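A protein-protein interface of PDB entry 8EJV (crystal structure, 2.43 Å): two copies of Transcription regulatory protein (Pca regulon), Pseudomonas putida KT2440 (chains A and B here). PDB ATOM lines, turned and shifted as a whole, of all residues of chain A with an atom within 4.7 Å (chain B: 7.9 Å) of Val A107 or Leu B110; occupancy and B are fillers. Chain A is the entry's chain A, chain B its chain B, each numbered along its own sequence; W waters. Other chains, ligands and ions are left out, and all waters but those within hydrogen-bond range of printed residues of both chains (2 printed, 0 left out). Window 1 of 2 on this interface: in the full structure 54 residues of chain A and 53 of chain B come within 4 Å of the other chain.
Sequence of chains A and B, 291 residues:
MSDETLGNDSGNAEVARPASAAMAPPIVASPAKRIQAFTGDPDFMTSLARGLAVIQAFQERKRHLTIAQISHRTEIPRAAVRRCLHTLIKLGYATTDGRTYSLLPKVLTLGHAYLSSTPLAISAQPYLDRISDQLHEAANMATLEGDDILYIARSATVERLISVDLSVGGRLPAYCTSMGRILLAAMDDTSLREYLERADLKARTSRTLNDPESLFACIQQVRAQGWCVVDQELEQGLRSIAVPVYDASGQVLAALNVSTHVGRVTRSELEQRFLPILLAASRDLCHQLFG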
ATOM      1  N   LEU A  52     -16.884   9.416 -11.196  1.00  0.00           N
ATOM      2  CA  LEU A  52     -18.173   8.796 -10.901  1.00  0.00           C
ATOM      3  C   LEU A  52     -19.249   9.271 -11.870  1.00  0.00           C
ATOM      4  O   LEU A  52     -20.073   8.470 -12.338  1.00  0.00           O
ATOM      5  CB  LEU A  52     -18.594   9.081  -9.462  1.00  0.00           C
ATOM      6  CG  LEU A  52     -17.702   8.420  -8.419  1.00  0.00           C
ATOM      7  CD1 LEU A  52     -17.657   9.281  -7.160  1.00  0.00           C
ATOM      8  CD2 LEU A  52     -18.178   7.011  -8.140  1.00  0.00           C
ATOM      9  N   ILE A  55     -18.972   7.262 -15.016  1.00  0.00           N
ATOM     10  CA  ILE A  55     -19.620   5.954 -14.924  1.00  0.00           C
ATOM     11  C   ILE A  55     -21.115   6.096 -15.161  1.00  0.00           C
ATOM     12  O   ILE A  55     -21.703   5.377 -15.975  1.00  0.00           O
ATOM     13  CB  ILE A  55     -19.334   5.284 -13.569  1.00  0.00           C
ATOM     14  CG1 ILE A  55     -17.863   4.875 -13.467  1.00  0.00           C
ATOM     15  CG2 ILE A  55     -20.232   4.057 -13.401  1.00  0.00           C
ATOM     16  CD1 ILE A  55     -17.437   4.448 -12.070  1.00  0.00           C
ATOM     17  N   GLN A  56     -21.746   7.051 -14.472  1.00  0.00           N
ATOM     18  CA  GLN A  56     -23.179   7.283 -14.631  1.00  0.00           C
ATOM     19  C   GLN A  56     -23.567   7.636 -16.062  1.00  0.00           C
ATOM     20  O   GLN A  56     -24.737   7.472 -16.435  1.00  0.00           O
ATOM     21  CB  GLN A  56     -23.643   8.414 -13.711  1.00  0.00           C
ATOM     22  CG  GLN A  56     -23.461   8.160 -12.229  1.00  0.00           C
ATOM     23  CD  GLN A  56     -24.425   7.123 -11.678  1.00  0.00           C
ATOM     24  OE1 GLN A  56     -25.293   6.613 -12.388  1.00  0.00           O
ATOM     25  NE2 GLN A  56     -24.288   6.826 -10.394  1.00  0.00           N
ATOM     26  N   TYR A  93     -11.854  -0.950 -14.778  1.00  0.00           N
ATOM     27  CA  TYR A  93     -13.280  -0.663 -14.785  1.00  0.00           C
ATOM     28  C   TYR A  93     -13.830  -0.423 -16.182  1.00  0.00           C
ATOM     29  O   TYR A  93     -15.052  -0.398 -16.348  1.00  0.00           O
ATOM     30  CB  TYR A  93     -13.592   0.557 -13.910  1.00  0.00           C
ATOM     31  CG  TYR A  93     -13.532   0.285 -12.427  1.00  0.00           C
ATOM     32  CD1 TYR A  93     -14.549  -0.427 -11.778  1.00  0.00           C
ATOM     33  CD2 TYR A  93     -12.455   0.744 -11.666  1.00  0.00           C
ATOM     34  CE1 TYR A  93     -14.492  -0.667 -10.416  1.00  0.00           C
ATOM     35  CE2 TYR A  93     -12.388   0.507 -10.313  1.00  0.00           C
ATOM     36  CZ  TYR A  93     -13.405  -0.199  -9.688  1.00  0.00           C
ATOM     37  OH  TYR A  93     -13.313  -0.430  -8.328  1.00  0.00           O
ATOM     38  N   LEU A 103     -18.054   0.108 -20.170  1.00  0.00           N
ATOM     39  CA  LEU A 103     -17.671  -0.280 -18.825  1.00  0.00           C
ATOM     40  C   LEU A 103     -17.359  -1.775 -18.782  1.00  0.00           C
ATOM     41  O   LEU A 103     -17.793  -2.549 -19.639  1.00  0.00           O
ATOM     42  CB  LEU A 103     -18.778   0.075 -17.828  1.00  0.00           C
ATOM     43  CG  LEU A 103     -19.157   1.556 -17.767  1.00  0.00           C
ATOM     44  CD1 LEU A 103     -20.304   1.811 -16.781  1.00  0.00           C
ATOM     45  CD2 LEU A 103     -17.942   2.401 -17.406  1.00  0.00           C
ATOM     46  N   LEU A 104     -16.585  -2.180 -17.755  1.00  0.00           N
ATOM     47  CA  LEU A 104     -16.192  -3.570 -17.503  1.00  0.00           C
ATOM     48  C   LEU A 104     -16.941  -4.146 -16.295  1.00  0.00           C
ATOM     49  O   LEU A 104     -17.386  -3.393 -15.421  1.00  0.00           O
ATOM     50  CB  LEU A 104     -14.679  -3.661 -17.267  1.00  0.00           C
ATOM     51  CG  LEU A 104     -13.798  -3.670 -18.519  1.00  0.00           C
ATOM     52  CD1 LEU A 104     -12.309  -3.732 -18.139  1.00  0.00           C
ATOM     53  CD2 LEU A 104     -14.167  -4.831 -19.444  1.00  0.00           C
ATOM     54  N   PRO A 105     -17.101  -5.489 -16.212  1.00  0.00           N
ATOM     55  CA  PRO A 105     -17.917  -6.071 -15.131  1.00  0.00           C
ATOM     56  C   PRO A 105     -17.483  -5.661 -13.735  1.00  0.00           C
ATOM     57  O   PRO A 105     -18.295  -5.656 -12.798  1.00  0.00           O
ATOM     58  CB  PRO A 105     -17.747  -7.581 -15.338  1.00  0.00           C
ATOM     59  CG  PRO A 105     -17.425  -7.745 -16.770  1.00  0.00           C
ATOM     60  CD  PRO A 105     -16.601  -6.532 -17.131  1.00  0.00           C
ATOM     61  N   LYS A 106     -16.204  -5.305 -13.586  1.00  0.00           N
ATOM     62  CA  LYS A 106     -15.711  -4.910 -12.273  1.00  0.00           C
ATOM     63  C   LYS A 106     -16.546  -3.782 -11.675  1.00  0.00           C
ATOM     64  O   LYS A 106     -16.663  -3.679 -10.448  1.00  0.00           O
ATOM     65  CB  LYS A 106     -14.247  -4.502 -12.364  1.00  0.00           C
ATOM     66  CG  LYS A 106     -13.604  -4.303 -11.019  1.00  0.00           C
ATOM     67  CD  LYS A 106     -12.182  -3.794 -11.155  1.00  0.00           C
ATOM     68  CE  LYS A 106     -11.546  -3.622  -9.785  1.00  0.00           C
ATOM     69  NZ  LYS A 106     -10.133  -3.216  -9.906  1.00  0.00           N
ATOM     70  N   VAL A 107     -17.166  -2.951 -12.515  1.00  0.00           N
ATOM     71  CA  VAL A 107     -18.045  -1.902 -11.996  1.00  0.00           C
ATOM     72  C   VAL A 107     -19.138  -2.499 -11.123  1.00  0.00           C
ATOM     73  O   VAL A 107     -19.548  -1.891 -10.125  1.00  0.00           O
ATOM     74  CB  VAL A 107     -18.640  -1.082 -13.157  1.00  0.00           C
ATOM     75  CG1 VAL A 107     -19.699  -0.128 -12.646  1.00  0.00           C
ATOM     76  CG2 VAL A 107     -17.545  -0.302 -13.858  1.00  0.00           C
ATOM     77  N   LEU A 108     -19.614  -3.700 -11.470  1.00  0.00           N
ATOM     78  CA  LEU A 108     -20.633  -4.360 -10.663  1.00  0.00           C
ATOM     79  C   LEU A 108     -20.169  -4.587  -9.238  1.00  0.00           C
ATOM     80  O   LEU A 108     -20.987  -4.538  -8.306  1.00  0.00           O
ATOM     81  CB  LEU A 108     -21.018  -5.698 -11.284  1.00  0.00           C
ATOM     82  CG  LEU A 108     -22.062  -5.683 -12.385  1.00  0.00           C
ATOM     83  CD1 LEU A 108     -22.184  -7.084 -12.949  1.00  0.00           C
ATOM     84  CD2 LEU A 108     -23.400  -5.190 -11.854  1.00  0.00           C
ATOM     85  N   THR A 109     -18.874  -4.859  -9.042  1.00  0.00           N
ATOM     86  CA  THR A 109     -18.411  -5.092  -7.680  1.00  0.00           C
ATOM     87  C   THR A 109     -18.585  -3.858  -6.803  1.00  0.00           C
ATOM     88  O   THR A 109     -18.636  -3.989  -5.575  1.00  0.00           O
ATOM     89  CB  THR A 109     -16.951  -5.545  -7.665  1.00  0.00           C
ATOM     90  OG1 THR A 109     -16.106  -4.484  -8.115  1.00  0.00           O
ATOM     91  CG2 THR A 109     -16.783  -6.748  -8.568  1.00  0.00           C
ATOM     92  N   LEU A 110     -18.693  -2.665  -7.398  1.00  0.00           N
ATOM     93  CA  LEU A 110     -18.956  -1.475  -6.599  1.00  0.00           C
ATOM     94  C   LEU A 110     -20.328  -1.564  -5.936  1.00  0.00           C
ATOM     95  O   LEU A 110     -20.473  -1.292  -4.739  1.00  0.00           O
ATOM     96  CB  LEU A 110     -18.848  -0.221  -7.466  1.00  0.00           C
ATOM     97  CG  LEU A 110     -17.453   0.206  -7.943  1.00  0.00           C
ATOM     98  CD1 LEU A 110     -17.570   1.325  -8.959  1.00  0.00           C
ATOM     99  CD2 LEU A 110     -16.557   0.635  -6.803  1.00  0.00           C
ATOM    100  N   GLY A 111     -21.354  -1.961  -6.694  1.00  0.00           N
ATOM    101  CA  GLY A 111     -22.664  -2.153  -6.092  1.00  0.00           C
ATOM    102  C   GLY A 111     -22.673  -3.254  -5.047  1.00  0.00           C
ATOM    103  O   GLY A 111     -23.404  -3.176  -4.060  1.00  0.00           O
ATOM    104  N   LEU B  52     -12.648   5.119  -5.616  1.00  0.00           N
ATOM    105  CA  LEU B  52     -13.214   3.827  -5.968  1.00  0.00           C
ATOM    106  C   LEU B  52     -12.723   2.747  -5.013  1.00  0.00           C
ATOM    107  O   LEU B  52     -13.508   1.901  -4.560  1.00  0.00           O
ATOM    108  CB  LEU B  52     -12.868   3.493  -7.417  1.00  0.00           C
ATOM    109  CG  LEU B  52     -13.450   4.465  -8.460  1.00  0.00           C
ATOM    110  CD1 LEU B  52     -12.910   4.161  -9.853  1.00  0.00           C
ATOM    111  CD2 LEU B  52     -14.986   4.461  -8.476  1.00  0.00           C
ATOM    112  N   ILE B  55     -14.607   2.852  -1.826  1.00  0.00           N
ATOM    113  CA  ILE B  55     -15.855   2.099  -1.962  1.00  0.00           C
ATOM    114  C   ILE B  55     -15.606   0.608  -1.781  1.00  0.00           C
ATOM    115  O   ILE B  55     -16.308  -0.066  -1.013  1.00  0.00           O
ATOM    116  CB  ILE B  55     -16.518   2.388  -3.316  1.00  0.00           C
ATOM    117  CG1 ILE B  55     -16.972   3.848  -3.371  1.00  0.00           C
ATOM    118  CG2 ILE B  55     -17.660   1.394  -3.562  1.00  0.00           C
ATOM    119  CD1 ILE B  55     -17.599   4.267  -4.680  1.00  0.00           C
ATOM    120  N   GLN B  56     -14.605   0.066  -2.483  1.00  0.00           N
ATOM    121  CA  GLN B  56     -14.334  -1.365  -2.411  1.00  0.00           C
ATOM    122  C   GLN B  56     -13.961  -1.818  -1.006  1.00  0.00           C
ATOM    123  O   GLN B  56     -14.082  -3.007  -0.694  1.00  0.00           O
ATOM    124  CB  GLN B  56     -13.204  -1.753  -3.376  1.00  0.00           C
ATOM    125  CG  GLN B  56     -13.522  -1.570  -4.855  1.00  0.00           C
ATOM    126  CD  GLN B  56     -14.525  -2.593  -5.374  1.00  0.00           C
ATOM    127  OE1 GLN B  56     -14.988  -3.465  -4.628  1.00  0.00           O
ATOM    128  NE2 GLN B  56     -14.872  -2.483  -6.659  1.00  0.00           N
ATOM    129  N   GLN B  59     -16.486  -4.047   1.160  1.00  0.00           N
ATOM    130  CA  GLN B  59     -16.891  -5.418   0.848  1.00  0.00           C
ATOM    131  C   GLN B  59     -16.894  -6.285   2.105  1.00  0.00           C
ATOM    132  O   GLN B  59     -15.898  -6.351   2.830  1.00  0.00           O
ATOM    133  CB  GLN B  59     -15.955  -6.039  -0.195  1.00  0.00           C
ATOM    134  CG  GLN B  59     -15.978  -5.374  -1.560  1.00  0.00           C
ATOM    135  CD  GLN B  59     -17.226  -5.690  -2.382  1.00  0.00           C
ATOM    136  OE1 GLN B  59     -18.114  -6.435  -1.951  1.00  0.00           O
ATOM    137  NE2 GLN B  59     -17.307  -5.095  -3.568  1.00  0.00           N
ATOM    138  N   LEU B  88     -17.636  11.493  -1.416  1.00  0.00           N
ATOM    139  CA  LEU B  88     -18.708  10.519  -1.585  1.00  0.00           C
ATOM    140  C   LEU B  88     -19.957  10.928  -0.822  1.00  0.00           C
ATOM    141  O   LEU B  88     -21.079  10.751  -1.315  1.00  0.00           O
ATOM    142  CB  LEU B  88     -18.246   9.136  -1.132  1.00  0.00           C
ATOM    143  CG  LEU B  88     -17.182   8.489  -2.017  1.00  0.00           C
ATOM    144  CD1 LEU B  88     -16.556   7.259  -1.349  1.00  0.00           C
ATOM    145  CD2 LEU B  88     -17.782   8.148  -3.378  1.00  0.00           C
ATOM    146  N   TYR B  93     -23.160   9.155  -2.177  1.00  0.00           N
ATOM    147  CA  TYR B  93     -22.761   7.753  -2.234  1.00  0.00           C
ATOM    148  C   TYR B  93     -22.435   7.165  -0.866  1.00  0.00           C
ATOM    149  O   TYR B  93     -22.305   5.945  -0.753  1.00  0.00           O
ATOM    150  CB  TYR B  93     -21.544   7.574  -3.146  1.00  0.00           C
ATOM    151  CG  TYR B  93     -21.829   7.750  -4.615  1.00  0.00           C
ATOM    152  CD1 TYR B  93     -22.477   6.756  -5.342  1.00  0.00           C
ATOM    153  CD2 TYR B  93     -21.430   8.904  -5.284  1.00  0.00           C
ATOM    154  CE1 TYR B  93     -22.729   6.912  -6.692  1.00  0.00           C
ATOM    155  CE2 TYR B  93     -21.678   9.074  -6.630  1.00  0.00           C
ATOM    156  CZ  TYR B  93     -22.330   8.079  -7.333  1.00  0.00           C
ATOM    157  OH  TYR B  93     -22.579   8.251  -8.679  1.00  0.00           O
ATOM    158  N   PRO B 105     -27.456   3.592  -0.743  1.00  0.00           N
ATOM    159  CA  PRO B 105     -27.910   2.740  -1.856  1.00  0.00           C
ATOM    160  C   PRO B 105     -27.526   3.259  -3.224  1.00  0.00           C
ATOM    161  O   PRO B 105     -27.433   2.459  -4.165  1.00  0.00           O
ATOM    162  CB  PRO B 105     -29.436   2.718  -1.688  1.00  0.00           C
ATOM    163  CG  PRO B 105     -29.678   3.022  -0.258  1.00  0.00           C
ATOM    164  CD  PRO B 105     -28.575   3.973   0.143  1.00  0.00           C
ATOM    165  N   LYS B 106     -27.297   4.566  -3.373  1.00  0.00           N
ATOM    166  CA  LYS B 106     -26.946   5.109  -4.677  1.00  0.00           C
ATOM    167  C   LYS B 106     -25.731   4.410  -5.282  1.00  0.00           C
ATOM    168  O   LYS B 106     -25.593   4.384  -6.512  1.00  0.00           O
ATOM    169  CB  LYS B 106     -26.719   6.620  -4.560  1.00  0.00           C
ATOM    170  CG  LYS B 106     -26.327   7.323  -5.864  1.00  0.00           C
ATOM    171  CD  LYS B 106     -25.911   8.772  -5.609  1.00  0.00           C
ATOM    172  CE  LYS B 106     -26.184   9.674  -6.797  1.00  0.00           C
ATOM    173  NZ  LYS B 106     -25.817  11.073  -6.464  1.00  0.00           N
ATOM    174  N   VAL B 107     -24.863   3.816  -4.457  1.00  0.00           N
ATOM    175  CA  VAL B 107     -23.754   3.019  -4.990  1.00  0.00           C
ATOM    176  C   VAL B 107     -24.265   1.930  -5.925  1.00  0.00           C
ATOM    177  O   VAL B 107     -23.602   1.583  -6.914  1.00  0.00           O
ATOM    178  CB  VAL B 107     -22.915   2.437  -3.827  1.00  0.00           C
ATOM    179  CG1 VAL B 107     -21.889   1.466  -4.331  1.00  0.00           C
ATOM    180  CG2 VAL B 107     -22.216   3.552  -3.076  1.00  0.00           C
ATOM    181  N   LEU B 108     -25.451   1.388  -5.641  1.00  0.00           N
ATOM    182  CA  LEU B 108     -26.026   0.347  -6.494  1.00  0.00           C
ATOM    183  C   LEU B 108     -26.201   0.808  -7.931  1.00  0.00           C
ATOM    184  O   LEU B 108     -26.151  -0.019  -8.848  1.00  0.00           O
ATOM    185  CB  LEU B 108     -27.379  -0.098  -5.947  1.00  0.00           C
ATOM    186  CG  LEU B 108     -27.263  -1.135  -4.850  1.00  0.00           C
ATOM    187  CD1 LEU B 108     -28.621  -1.402  -4.255  1.00  0.00           C
ATOM    188  CD2 LEU B 108     -26.649  -2.402  -5.418  1.00  0.00           C
ATOM    189  N   THR B 109     -26.450   2.104  -8.147  1.00  0.00           N
ATOM    190  CA  THR B 109     -26.679   2.584  -9.502  1.00  0.00           C
ATOM    191  C   THR B 109     -25.414   2.541 -10.340  1.00  0.00           C
ATOM    192  O   THR B 109     -25.505   2.498 -11.571  1.00  0.00           O
ATOM    193  CB  THR B 109     -27.237   4.007  -9.504  1.00  0.00           C
ATOM    194  OG1 THR B 109     -26.189   4.924  -9.170  1.00  0.00           O
ATOM    195  CG2 THR B 109     -28.354   4.147  -8.489  1.00  0.00           C
ATOM    196  N   LEU B 110     -24.237   2.537  -9.707  1.00  0.00           N
ATOM    197  CA  LEU B 110     -22.996   2.397 -10.463  1.00  0.00           C
ATOM    198  C   LEU B 110     -22.972   1.075 -11.218  1.00  0.00           C
ATOM    199  O   LEU B 110     -22.681   1.034 -12.419  1.00  0.00           O
ATOM    200  CB  LEU B 110     -21.784   2.522  -9.536  1.00  0.00           C
ATOM    201  CG  LEU B 110     -21.563   3.886  -8.869  1.00  0.00           C
ATOM    202  CD1 LEU B 110     -20.415   3.841  -7.850  1.00  0.00           C
ATOM    203  CD2 LEU B 110     -21.328   4.970  -9.912  1.00  0.00           C
ATOM    204  N   GLY B 111     -23.302  -0.020 -10.530  1.00  0.00           N
ATOM    205  CA  GLY B 111     -23.399  -1.297 -11.210  1.00  0.00           C
ATOM    206  C   GLY B 111     -24.477  -1.312 -12.273  1.00  0.00           C
ATOM    207  O   GLY B 111     -24.315  -1.947 -13.322  1.00  0.00           O
ATOM    208  N   HIS B 112     -25.592  -0.627 -12.018  1.00  0.00           N
ATOM    209  CA  HIS B 112     -26.653  -0.545 -13.013  1.00  0.00           C
ATOM    210  C   HIS B 112     -26.158   0.116 -14.299  1.00  0.00           C
ATOM    211  O   HIS B 112     -26.655  -0.185 -15.389  1.00  0.00           O
ATOM    212  CB  HIS B 112     -27.840   0.207 -12.417  1.00  0.00           C
ATOM    213  CG  HIS B 112     -29.074   0.157 -13.256  1.00  0.00           C
ATOM    214  ND1 HIS B 112     -29.356   1.097 -14.224  1.00  0.00           N
ATOM    215  CD2 HIS B 112     -30.112  -0.711 -13.262  1.00  0.00           C
ATOM    216  CE1 HIS B 112     -30.511   0.806 -14.794  1.00  0.00           C
ATOM    217  NE2 HIS B 112     -30.988  -0.291 -14.232  1.00  0.00           N
ATOM    218  N   ALA B 113     -25.165   1.001 -14.195  1.00  0.00           N
ATOM    219  CA  ALA B 113     -24.613   1.624 -15.391  1.00  0.00           C
ATOM    220  C   ALA B 113     -23.873   0.612 -16.245  1.00  0.00           C
ATOM    221  O   ALA B 113     -23.910   0.701 -17.482  1.00  0.00           O
ATOM    222  CB  ALA B 113     -23.689   2.784 -15.014  1.00  0.00           C
ATOM    223  N   TYR B 114     -23.209  -0.358 -15.616  1.00  0.00           N
ATOM    224  CA  TYR B 114     -22.599  -1.431 -16.389  1.00  0.00           C
ATOM    225  C   TYR B 114     -23.661  -2.322 -17.017  1.00  0.00           C
ATOM    226  O   TYR B 114     -23.551  -2.685 -18.193  1.00  0.00           O
ATOM    227  CB  TYR B 114     -21.663  -2.272 -15.512  1.00  0.00           C
ATOM    228  CG  TYR B 114     -21.316  -3.587 -16.170  1.00  0.00           C
ATOM    229  CD1 TYR B 114     -20.297  -3.666 -17.111  1.00  0.00           C
ATOM    230  CD2 TYR B 114     -22.047  -4.740 -15.893  1.00  0.00           C
ATOM    231  CE1 TYR B 114     -20.008  -4.860 -17.729  1.00  0.00           C
ATOM    232  CE2 TYR B 114     -21.767  -5.922 -16.510  1.00  0.00           C
ATOM    233  CZ  TYR B 114     -20.754  -5.982 -17.429  1.00  0.00           C
ATOM    234  OH  TYR B 114     -20.468  -7.180 -18.038  1.00  0.00           O
ATOM    235  N   LEU B 115     -24.687  -2.707 -16.246  1.00  0.00           N
ATOM    236  CA  LEU B 115     -25.637  -3.693 -16.755  1.00  0.00           C
ATOM    237  C   LEU B 115     -26.503  -3.138 -17.876  1.00  0.00           C
ATOM    238  O   LEU B 115     -26.924  -3.896 -18.754  1.00  0.00           O
ATOM    239  CB  LEU B 115     -26.541  -4.216 -15.637  1.00  0.00           C
ATOM    240  CG  LEU B 115     -25.896  -5.110 -14.575  1.00  0.00           C
ATOM    241  CD1 LEU B 115     -26.850  -5.295 -13.407  1.00  0.00           C
ATOM    242  CD2 LEU B 115     -25.453  -6.453 -15.156  1.00  0.00           C
ATOM    243  N   SER B 116     -26.808  -1.845 -17.855  1.00  0.00           N
ATOM    244  CA  SER B 116     -27.713  -1.280 -18.843  1.00  0.00           C
ATOM    245  C   SER B 116     -26.982  -0.678 -20.038  1.00  0.00           C
ATOM    246  O   SER B 116     -27.615  -0.003 -20.857  1.00  0.00           O
ATOM    247  CB  SER B 116     -28.621  -0.228 -18.194  1.00  0.00           C
ATOM    248  OG  SER B 116     -27.878   0.755 -17.514  1.00  0.00           O
ATOM    249  N   SER B 117     -25.672  -0.917 -20.163  1.00  0.00           N
ATOM    250  CA  SER B 117     -24.902  -0.402 -21.288  1.00  0.00           C
ATOM    251  C   SER B 117     -23.989  -1.461 -21.900  1.00  0.00           C
ATOM    252  O   SER B 117     -23.061  -1.117 -22.638  1.00  0.00           O
ATOM    253  CB  SER B 117     -24.091   0.828 -20.869  1.00  0.00           C
ATOM    254  OG  SER B 117     -23.052   0.511 -19.964  1.00  0.00           O
ATOM    255  N   GLU B 145     -12.538 -12.057 -12.971  1.00  0.00           N
ATOM    256  CA  GLU B 145     -12.118 -10.801 -12.355  1.00  0.00           C
ATOM    257  C   GLU B 145     -10.991 -11.131 -11.377  1.00  0.00           C
ATOM    258  O   GLU B 145     -11.224 -11.711 -10.314  1.00  0.00           O
ATOM    259  CB  GLU B 145     -13.304 -10.106 -11.682  1.00  0.00           C
ATOM    260  CG  GLU B 145     -12.978  -9.179 -10.519  1.00  0.00           C
ATOM    261  CD  GLU B 145     -12.291  -7.910 -10.944  1.00  0.00           C
ATOM    262  OE1 GLU B 145     -12.410  -7.540 -12.132  1.00  0.00           O
ATOM    263  OE2 GLU B 145     -11.634  -7.284 -10.085  1.00  0.00           O
ATOM    264  N   LEU B 150     -16.840 -13.530 -11.477  1.00  0.00           N
ATOM    265  CA  LEU B 150     -17.730 -12.427 -11.134  1.00  0.00           C
ATOM    266  C   LEU B 150     -19.077 -12.706 -11.779  1.00  0.00           C
ATOM    267  O   LEU B 150     -19.163 -12.809 -13.007  1.00  0.00           O
ATOM    268  CB  LEU B 150     -17.172 -11.095 -11.652  1.00  0.00           C
ATOM    269  CG  LEU B 150     -17.586  -9.753 -11.045  1.00  0.00           C
ATOM    270  CD1 LEU B 150     -16.777  -8.632 -11.695  1.00  0.00           C
ATOM    271  CD2 LEU B 150     -19.055  -9.490 -11.220  1.00  0.00           C
ATOM    272  N   GLY B 169     -22.820  -9.276  -9.023  1.00  0.00           N
ATOM    273  CA  GLY B 169     -21.721  -8.493  -8.505  1.00  0.00           C
ATOM    274  C   GLY B 169     -20.867  -9.231  -7.503  1.00  0.00           C
ATOM    275  O   GLY B 169     -19.841  -8.695  -7.074  1.00  0.00           O
HETATM  276  O   HOH W   1     -20.688  -0.432 -20.887  1.00  0.00           O
HETATM  277  O   HOH W   2     -14.037  -6.544 -14.877  1.00  0.00           O
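Printed residues of chain B that touch a printed residue of chain A: Leu B52, Ile B55, Gln B56, Gln B59, Leu B88, Tyr B93, Val B107, Leu B108, Thr B109, Leu B110, Gly B111, Ala B113, Tyr B114, Leu B115, Glu B145, Leu B150 and Gly B169.
Hydrophobic or aromatic side chains of chain A within 4 Å of the printed part of chain B: Leu A52, Ile A55, Tyr A93, Leu A103, Pro A105, Val A107, Leu A108 and Leu A110.
Among the printed residues, 31 pairs touch across the chains.
Among the printed residues, no Asp or Glu carboxylate lies within 4 Å of a Lys or Arg side-chain nitrogen of the other chain.
Among the printed residues, pairs that only touch across the chains: Leu A110 with Val B107 (3.1 Å), Val A107 with Leu B110 (3.2 Å), Pro A105 with Tyr B114 (3.3 Å), Leu A104 with Tyr B114 (3.4 Å), Ile A55 with Ala B113 (3.4 Å), Leu A110 with Ile B55 (3.5 Å), Pro A105 with Leu B150 (3.5 Å), Gln A56 with Leu B110 (3.5 Å), Leu A110 with Gln B56 (3.5 Å), Lys A106 with Glu B145 (3.6 Å), Gly A111 with Leu B108 (3.6 Å), Leu A108 with Tyr B114 (3.6 Å), Thr A109 with Leu B150 (3.7 Å), Leu A108 with Gly B111 (3.7 Å), Leu A108 with Leu B115 (3.7 Å), Tyr A93 with Leu B52 (3.7 Å), Leu A103 with Tyr B114 (3.7 Å), Ile A55 with Leu B110 (3.8 Å), Leu A103 with Ala B113 (3.8 Å), Lys A106 with Leu B150 (3.9 Å), Leu A52 with Leu B110 (3.9 Å), Thr A109 with Gly B169 (3.9 Å), Gly A111 with Val B107 (3.9 Å), Leu A52 with Leu B88 (3.95 Å), Leu A110 with Leu B110 (3.96 Å) and Leu A110 with Leu B52 (3.99 Å).
O of Tyr A93 sits at hydrogen-bond distance from N of Leu A104, at 2.7 Å.
N of Tyr B93 is in hydrogen-bond range of O of Leu B88 (2.8 Å).
OG1 of Thr B109 sits at hydrogen-bond distance from O of Lys B106, 2.8 Å away.
The side-chain hydroxyl of Ser B117 lies within hydrogen-bond range of the backbone carbonyl oxygen of Ala B113 (2.6 Å).
The side-chain amide oxygen (OE1) of Gln B56 is in hydrogen-bond range of the side-chain amide nitrogen (NE2) of Gln B59.
O of Lys A106 lies within hydrogen-bond range of OG1 of Thr A109, at 2.5 Å.
The side-chain hydroxyl (OG1) of Thr A109 is in hydrogen-bond range of the side-chain amide nitrogen (NE2) of Gln B56, at 2.8 Å.
The side-chain amide nitrogen (NE2) of Gln A56 lies within hydrogen-bond range of the side-chain hydroxyl (OH) of Tyr B93 (2.8 Å).
NE2 of Gln B59 lies within hydrogen-bond range of O of Thr A109 (2.6 Å).
The side-chain hydroxyl (OH) of Tyr A93 is in hydrogen-bond range of the side-chain amide nitrogen (NE2) of Gln B56 (3.1 Å).
The side-chain hydroxyl of Thr B109 lies within hydrogen-bond range of the side-chain amide nitrogen of Gln A56 (3.0 Å).
Of the printed residues of chain B, Gln A56 touches Tyr B93 (2.8 Å), Thr B109 (3.0 Å) and Leu B110 (3.5 Å).
Of the printed residues of chain B, Val A107 touches Leu B110.
Lys B106 touches none of the printed residues of chain A.
Printed residues of chain A within 4 Å of Val B107: Leu A110 (3.1 Å) and Gly A111 (3.9 Å).
Leu B110 touches just these residues of chain A: Leu A52 (3.9 Å), Ile A55 (3.8 Å), Gln A56 (3.5 Å), Val A107 (3.2 Å) and Leu A110 (3.96 Å).
Printed residues of chain A within 4 Å of Tyr B114: Leu A103 (3.7 Å), Leu A104 (3.4 Å), Pro A105 (3.3 Å) and Leu A108 (3.6 Å).
Ser B117 touches none of the printed residues of chain A.
The nearest printed residue of chain B that does not touch Ile A55 is Leu B52 (4.4 Å).
Water W1 lies within hydrogen-bond range of the side-chain hydroxyl of Ser B117 (2.7 Å) and the backbone NH of Leu A103 (2.8 Å).
Water W2 bridges N of Lys A106 (2.8 Å) and OE1 of Glu B145 (3.3 Å).
Gln A56 touches Tyr B93, and with the chains exchanged Tyr A93 touches Gln B56.
Gln A56 touches Leu B110, and with the chains exchanged Leu A110 touches Gln B56.
Leu A108 touches Gly B111, and with the chains exchanged Gly A111 touches Leu B108.
Gly A111 touches Val B107, but with the chains exchanged Val A107 does not touch Gly B111 (4.04 Å).
Positions printed for both chains: 52, 55, 56, 93, 105, 106, 107, 108, 109, 110 and 111.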
